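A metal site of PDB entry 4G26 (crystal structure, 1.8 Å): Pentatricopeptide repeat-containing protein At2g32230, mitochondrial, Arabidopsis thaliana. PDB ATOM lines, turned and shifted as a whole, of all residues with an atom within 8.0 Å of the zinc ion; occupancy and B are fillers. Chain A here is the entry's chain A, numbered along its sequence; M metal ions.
Within 4 Å of the zinc ion: Cys 273, Cys 276, His 477 and Cys 494. The nearest printed residue that does not touch the zinc ion is Cys 275 (4.4 Å).
The backbone NH (N) of Glu 278 sits close to the side-chain sulfur (SG) of Cys 276 (3.5 Å). N of Cys 494 is in hydrogen-bond range of O of Lys 263 (2.9 Å). The side-chain sulfur (SG) of Cys 273 lies close to the backbone NH (N) of Cys 275. N of Cys 273 is in hydrogen-bond range of O of Glu 278, 2.8 Å away. SD of Met 267 lies close to N of Cys 273, 3.5 Å away.
The zinc ion is bound by a ring nitrogen (NE2) of His 477 (2.1 Å), the side-chain sulfur of Cys 276 (2.3 Å), the side-chain sulfur of Cys 494 (2.4 Å) and the side-chain sulfur of Cys 273 (2.4 Å).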
ATOM      1  N   ASN A 261      -9.084  -4.979  19.127  1.00  0.00           N
ATOM      2  CA  ASN A 261     -10.040  -3.930  18.718  1.00  0.00           C
ATOM      3  C   ASN A 261     -11.435  -4.536  18.691  1.00  0.00           C
ATOM      4  O   ASN A 261     -11.701  -5.510  18.007  1.00  0.00           O
ATOM      5  CB  ASN A 261      -9.654  -3.296  17.373  1.00  0.00           C
ATOM      6  CG  ASN A 261      -8.416  -2.424  17.494  1.00  0.00           C
ATOM      7  OD1 ASN A 261      -7.485  -2.531  16.691  1.00  0.00           O
ATOM      8  ND2 ASN A 261      -8.379  -1.555  18.515  1.00  0.00           N
ATOM      9  N   LYS A 263     -15.490  -3.911  18.400  1.00  0.00           N
ATOM     10  CA  LYS A 263     -16.493  -2.946  17.906  1.00  0.00           C
ATOM     11  C   LYS A 263     -17.856  -3.576  17.774  1.00  0.00           C
ATOM     12  O   LYS A 263     -17.976  -4.742  17.365  1.00  0.00           O
ATOM     13  CB  LYS A 263     -16.105  -2.370  16.535  1.00  0.00           C
ATOM     14  CG  LYS A 263     -14.729  -1.696  16.468  1.00  0.00           C
ATOM     15  CD  LYS A 263     -14.574  -0.423  17.307  1.00  0.00           C
ATOM     16  CE  LYS A 263     -13.091  -0.092  17.495  1.00  0.00           C
ATOM     17  NZ  LYS A 263     -12.830   0.732  18.720  1.00  0.00           N
ATOM     18  N   THR A 265     -20.970  -3.833  15.553  1.00  0.00           N
ATOM     19  CA  THR A 265     -21.094  -3.599  14.123  1.00  0.00           C
ATOM     20  C   THR A 265     -22.280  -4.416  13.581  1.00  0.00           C
ATOM     21  O   THR A 265     -23.077  -4.926  14.360  1.00  0.00           O
ATOM     22  CB  THR A 265     -19.766  -3.957  13.394  1.00  0.00           C
ATOM     23  OG1 THR A 265     -19.881  -3.562  12.018  1.00  0.00           O
ATOM     24  CG2 THR A 265     -19.464  -5.451  13.462  1.00  0.00           C
ATOM     25  N   GLU A 266     -22.397  -4.519  12.241  1.00  0.00           N
ATOM     26  CA  GLU A 266     -23.422  -5.213  11.550  1.00  0.00           C
ATOM     27  C   GLU A 266     -22.800  -5.936  10.389  1.00  0.00           C
ATOM     28  O   GLU A 266     -21.713  -5.563   9.952  1.00  0.00           O
ATOM     29  CB  GLU A 266     -24.495  -4.267  10.998  1.00  0.00           C
ATOM     30  CG  GLU A 266     -25.499  -3.788  12.030  1.00  0.00           C
ATOM     31  CD  GLU A 266     -26.312  -2.609  11.553  1.00  0.00           C
ATOM     32  OE1 GLU A 266     -26.207  -2.248  10.372  1.00  0.00           O
ATOM     33  OE2 GLU A 266     -27.077  -2.046  12.366  1.00  0.00           O
ATOM     34  N   MET A 267     -23.477  -6.965   9.877  1.00  0.00           N
ATOM     35  CA  MET A 267     -23.082  -7.605   8.637  1.00  0.00           C
ATOM     36  C   MET A 267     -23.985  -7.021   7.570  1.00  0.00           C
ATOM     37  O   MET A 267     -25.186  -6.779   7.798  1.00  0.00           O
ATOM     38  CB  MET A 267     -23.285  -9.136   8.704  1.00  0.00           C
ATOM     39  CG  MET A 267     -22.424  -9.868   9.720  1.00  0.00           C
ATOM     40  SD  MET A 267     -20.624  -9.721   9.670  1.00  0.00           S
ATOM     41  CE  MET A 267     -20.381  -8.885  11.249  1.00  0.00           C
ATOM     42  N   VAL A 272     -20.680  -9.690   4.989  1.00  0.00           N
ATOM     43  CA  VAL A 272     -19.455  -8.938   5.140  1.00  0.00           C
ATOM     44  C   VAL A 272     -19.539  -7.992   6.357  1.00  0.00           C
ATOM     45  O   VAL A 272     -20.440  -7.146   6.439  1.00  0.00           O
ATOM     46  CB  VAL A 272     -19.084  -8.129   3.861  1.00  0.00           C
ATOM     47  CG1 VAL A 272     -17.763  -7.384   4.086  1.00  0.00           C
ATOM     48  CG2 VAL A 272     -18.974  -9.051   2.665  1.00  0.00           C
ATOM     49  N   CYS A 273     -18.586  -8.138   7.280  1.00  0.00           N
ATOM     50  CA  CYS A 273     -18.518  -7.323   8.485  1.00  0.00           C
ATOM     51  C   CYS A 273     -18.267  -5.842   8.110  1.00  0.00           C
ATOM     52  O   CYS A 273     -17.344  -5.567   7.382  1.00  0.00           O
ATOM     53  CB  CYS A 273     -17.363  -7.827   9.403  1.00  0.00           C
ATOM     54  SG  CYS A 273     -17.113  -6.771  10.851  1.00  0.00           S
ATOM     55  N   LYS A 274     -19.101  -4.940   8.585  1.00  0.00           N
ATOM     56  CA  LYS A 274     -18.948  -3.521   8.210  1.00  0.00           C
ATOM     57  C   LYS A 274     -17.708  -2.880   8.874  1.00  0.00           C
ATOM     58  O   LYS A 274     -17.181  -1.882   8.377  1.00  0.00           O
ATOM     59  CB  LYS A 274     -20.209  -2.758   8.539  1.00  0.00           C
ATOM     60  CG  LYS A 274     -21.288  -3.046   7.485  1.00  0.00           C
ATOM     61  CD  LYS A 274     -22.569  -2.323   7.852  1.00  0.00           C
ATOM     62  CE  LYS A 274     -23.755  -2.865   7.043  1.00  0.00           C
ATOM     63  NZ  LYS A 274     -25.014  -2.335   7.643  1.00  0.00           N
ATOM     64  N   CYS A 275     -17.221  -3.483   9.956  1.00  0.00           N
ATOM     65  CA  CYS A 275     -16.036  -3.002  10.659  1.00  0.00           C
ATOM     66  C   CYS A 275     -14.748  -3.408   9.917  1.00  0.00           C
ATOM     67  O   CYS A 275     -14.015  -2.545   9.466  1.00  0.00           O
ATOM     68  CB  CYS A 275     -16.040  -3.541  12.079  1.00  0.00           C
ATOM     69  SG  CYS A 275     -14.592  -3.039  13.039  1.00  0.00           S
ATOM     70  N   CYS A 276     -14.511  -4.706   9.736  1.00  0.00           N
ATOM     71  CA  CYS A 276     -13.223  -5.209   9.237  1.00  0.00           C
ATOM     72  C   CYS A 276     -13.252  -5.820   7.826  1.00  0.00           C
ATOM     73  O   CYS A 276     -12.213  -6.262   7.308  1.00  0.00           O
ATOM     74  CB  CYS A 276     -12.636  -6.234  10.234  1.00  0.00           C
ATOM     75  SG  CYS A 276     -13.422  -7.895  10.135  1.00  0.00           S
ATOM     76  N   LYS A 277     -14.435  -5.912   7.238  1.00  0.00           N
ATOM     77  CA  LYS A 277     -14.651  -6.413   5.869  1.00  0.00           C
ATOM     78  C   LYS A 277     -14.389  -7.912   5.697  1.00  0.00           C
ATOM     79  O   LYS A 277     -14.267  -8.407   4.579  1.00  0.00           O
ATOM     80  CB  LYS A 277     -13.837  -5.614   4.813  1.00  0.00           C
ATOM     81  CG  LYS A 277     -13.942  -4.095   4.926  1.00  0.00           C
ATOM     82  CD  LYS A 277     -15.365  -3.592   5.141  1.00  0.00           C
ATOM     83  CE  LYS A 277     -15.409  -2.068   5.029  1.00  0.00           C
ATOM     84  NZ  LYS A 277     -16.806  -1.512   5.187  1.00  0.00           N
ATOM     85  N   GLU A 278     -14.320  -8.659   6.803  1.00  0.00           N
ATOM     86  CA  GLU A 278     -14.265 -10.095   6.680  1.00  0.00           C
ATOM     87  C   GLU A 278     -15.640 -10.564   6.162  1.00  0.00           C
ATOM     88  O   GLU A 278     -16.687 -10.096   6.612  1.00  0.00           O
ATOM     89  CB  GLU A 278     -13.897 -10.760   8.016  1.00  0.00           C
ATOM     90  CG  GLU A 278     -14.034 -12.279   7.999  1.00  0.00           C
ATOM     91  CD  GLU A 278     -12.863 -13.000   8.665  1.00  0.00           C
ATOM     92  OE1 GLU A 278     -12.231 -12.433   9.571  1.00  0.00           O
ATOM     93  OE2 GLU A 278     -12.558 -14.137   8.262  1.00  0.00           O
ATOM     94  N   LYS A 279     -15.603 -11.475   5.202  1.00  0.00           N
ATOM     95  CA  LYS A 279     -16.828 -12.146   4.756  1.00  0.00           C
ATOM     96  C   LYS A 279     -17.043 -13.428   5.570  1.00  0.00           C
ATOM     97  O   LYS A 279     -16.283 -14.378   5.507  1.00  0.00           O
ATOM     98  CB  LYS A 279     -16.814 -12.459   3.248  1.00  0.00           C
ATOM     99  CG  LYS A 279     -18.150 -13.091   2.783  1.00  0.00           C
ATOM    100  CD  LYS A 279     -18.367 -13.010   1.255  1.00  0.00           C
ATOM    101  CE  LYS A 279     -17.399 -13.925   0.488  1.00  0.00           C
ATOM    102  NZ  LYS A 279     -17.761 -15.360   0.683  1.00  0.00           N
ATOM    103  N   LEU A 280     -18.119 -13.462   6.339  1.00  0.00           N
ATOM    104  CA  LEU A 280     -18.441 -14.690   7.094  1.00  0.00           C
ATOM    105  C   LEU A 280     -18.741 -15.918   6.218  1.00  0.00           C
ATOM    106  O   LEU A 280     -19.155 -15.805   5.057  1.00  0.00           O
ATOM    107  CB  LEU A 280     -19.621 -14.454   8.025  1.00  0.00           C
ATOM    108  CG  LEU A 280     -19.427 -13.325   9.040  1.00  0.00           C
ATOM    109  CD1 LEU A 280     -20.517 -13.381  10.089  1.00  0.00           C
ATOM    110  CD2 LEU A 280     -18.039 -13.352   9.714  1.00  0.00           C
ATOM    111  N   THR A 475      -9.673 -14.018  14.428  1.00  0.00           N
ATOM    112  CA  THR A 475     -10.710 -12.968  14.538  1.00  0.00           C
ATOM    113  C   THR A 475     -12.070 -13.564  14.872  1.00  0.00           C
ATOM    114  O   THR A 475     -12.409 -14.598  14.327  1.00  0.00           O
ATOM    115  CB  THR A 475     -10.808 -12.174  13.217  1.00  0.00           C
ATOM    116  OG1 THR A 475      -9.512 -11.655  12.890  1.00  0.00           O
ATOM    117  CG2 THR A 475     -11.867 -11.032  13.286  1.00  0.00           C
ATOM    118  N   TRP A 476     -12.837 -12.893  15.735  1.00  0.00           N
ATOM    119  CA  TRP A 476     -14.125 -13.373  16.196  1.00  0.00           C
ATOM    120  C   TRP A 476     -15.238 -12.457  15.755  1.00  0.00           C
ATOM    121  O   TRP A 476     -15.079 -11.228  15.734  1.00  0.00           O
ATOM    122  CB  TRP A 476     -14.162 -13.473  17.678  1.00  0.00           C
ATOM    123  CG  TRP A 476     -13.321 -14.581  18.219  1.00  0.00           C
ATOM    124  CD1 TRP A 476     -11.944 -14.596  18.453  1.00  0.00           C
ATOM    125  CD2 TRP A 476     -13.793 -15.895  18.604  1.00  0.00           C
ATOM    126  NE1 TRP A 476     -11.550 -15.826  18.941  1.00  0.00           N
ATOM    127  CE2 TRP A 476     -12.634 -16.648  19.057  1.00  0.00           C
ATOM    128  CE3 TRP A 476     -15.049 -16.525  18.596  1.00  0.00           C
ATOM    129  CZ2 TRP A 476     -12.744 -17.971  19.488  1.00  0.00           C
ATOM    130  CZ3 TRP A 476     -15.140 -17.837  19.058  1.00  0.00           C
ATOM    131  CH2 TRP A 476     -14.016 -18.524  19.498  1.00  0.00           C
ATOM    132  N   HIS A 477     -16.339 -13.074  15.346  1.00  0.00           N
ATOM    133  CA  HIS A 477     -17.604 -12.364  15.087  1.00  0.00           C
ATOM    134  C   HIS A 477     -18.673 -13.028  15.890  1.00  0.00           C
ATOM    135  O   HIS A 477     -18.929 -14.226  15.708  1.00  0.00           O
ATOM    136  CB  HIS A 477     -17.899 -12.337  13.609  1.00  0.00           C
ATOM    137  CG  HIS A 477     -16.931 -11.491  12.819  1.00  0.00           C
ATOM    138  ND1 HIS A 477     -15.807 -11.995  12.291  1.00  0.00           N
ATOM    139  CD2 HIS A 477     -16.908 -10.111  12.550  1.00  0.00           C
ATOM    140  CE1 HIS A 477     -15.128 -11.014  11.672  1.00  0.00           C
ATOM    141  NE2 HIS A 477     -15.794  -9.868  11.837  1.00  0.00           N
ATOM    142  N   VAL A 478     -19.326 -12.263  16.774  1.00  0.00           N
ATOM    143  CA  VAL A 478     -20.347 -12.803  17.675  1.00  0.00           C
ATOM    144  C   VAL A 478     -21.710 -12.106  17.442  1.00  0.00           C
ATOM    145  O   VAL A 478     -21.834 -10.899  17.638  1.00  0.00           O
ATOM    146  CB  VAL A 478     -19.927 -12.607  19.145  1.00  0.00           C
ATOM    147  CG1 VAL A 478     -21.048 -13.052  20.112  1.00  0.00           C
ATOM    148  CG2 VAL A 478     -18.561 -13.308  19.429  1.00  0.00           C
ATOM    149  N   TRP A 492     -23.636  -7.223  16.020  1.00  0.00           N
ATOM    150  CA  TRP A 492     -22.568  -8.194  16.107  1.00  0.00           C
ATOM    151  C   TRP A 492     -21.424  -7.569  16.825  1.00  0.00           C
ATOM    152  O   TRP A 492     -21.299  -6.320  16.839  1.00  0.00           O
ATOM    153  CB  TRP A 492     -22.077  -8.552  14.726  1.00  0.00           C
ATOM    154  CG  TRP A 492     -22.973  -9.434  13.929  1.00  0.00           C
ATOM    155  CD1 TRP A 492     -24.198  -9.119  13.290  1.00  0.00           C
ATOM    156  CD2 TRP A 492     -22.729 -10.838  13.596  1.00  0.00           C
ATOM    157  NE1 TRP A 492     -24.694 -10.205  12.620  1.00  0.00           N
ATOM    158  CE2 TRP A 492     -23.859 -11.273  12.753  1.00  0.00           C
ATOM    159  CE3 TRP A 492     -21.726 -11.753  13.893  1.00  0.00           C
ATOM    160  CZ2 TRP A 492     -23.955 -12.559  12.261  1.00  0.00           C
ATOM    161  CZ3 TRP A 492     -21.812 -13.044  13.370  1.00  0.00           C
ATOM    162  CH2 TRP A 492     -22.907 -13.444  12.568  1.00  0.00           C
ATOM    163  N   LEU A 493     -20.569  -8.403  17.421  1.00  0.00           N
ATOM    164  CA  LEU A 493     -19.318  -7.930  17.948  1.00  0.00           C
ATOM    165  C   LEU A 493     -18.230  -8.365  16.965  1.00  0.00           C
ATOM    166  O   LEU A 493     -18.214  -9.548  16.506  1.00  0.00           O
ATOM    167  CB  LEU A 493     -19.080  -8.556  19.325  1.00  0.00           C
ATOM    168  CG  LEU A 493     -18.067  -7.820  20.193  1.00  0.00           C
ATOM    169  CD1 LEU A 493     -18.629  -6.479  20.660  1.00  0.00           C
ATOM    170  CD2 LEU A 493     -17.668  -8.700  21.376  1.00  0.00           C
ATOM    171  N   CYS A 494     -17.376  -7.431  16.582  1.00  0.00           N
ATOM    172  CA  CYS A 494     -16.149  -7.748  15.843  1.00  0.00           C
ATOM    173  C   CYS A 494     -14.937  -7.581  16.757  1.00  0.00           C
ATOM    174  O   CYS A 494     -14.669  -6.471  17.222  1.00  0.00           O
ATOM    175  CB  CYS A 494     -16.002  -6.791  14.652  1.00  0.00           C
ATOM    176  SG  CYS A 494     -14.449  -6.903  13.709  1.00  0.00           S
ATOM    177  N   ALA A 495     -14.204  -8.672  17.005  1.00  0.00           N
ATOM    178  CA  ALA A 495     -13.005  -8.645  17.858  1.00  0.00           C
ATOM    179  C   ALA A 495     -11.823  -9.097  17.038  1.00  0.00           C
ATOM    180  O   ALA A 495     -11.769 -10.258  16.649  1.00  0.00           O
ATOM    181  CB  ALA A 495     -13.182  -9.551  19.085  1.00  0.00           C
ATOM    182  N   LYS A 496     -10.892  -8.169  16.771  1.00  0.00           N
ATOM    183  CA  LYS A 496      -9.781  -8.410  15.855  1.00  0.00           C
ATOM    184  C   LYS A 496      -8.499  -7.822  16.521  1.00  0.00           C
ATOM    185  O   LYS A 496      -8.583  -6.732  17.037  1.00  0.00           O
ATOM    186  CB  LYS A 496     -10.027  -7.649  14.540  1.00  0.00           C
ATOM    187  CG  LYS A 496      -9.026  -7.937  13.455  1.00  0.00           C
ATOM    188  CD  LYS A 496      -9.472  -7.340  12.119  1.00  0.00           C
ATOM    189  CE  LYS A 496      -8.521  -7.780  11.003  1.00  0.00           C
ATOM    190  NZ  LYS A 496      -8.666  -9.252  10.819  1.00  0.00           N
HETATM  191 ZN    ZN M   1     -15.130  -7.845  11.655  1.00  0.00          ZN
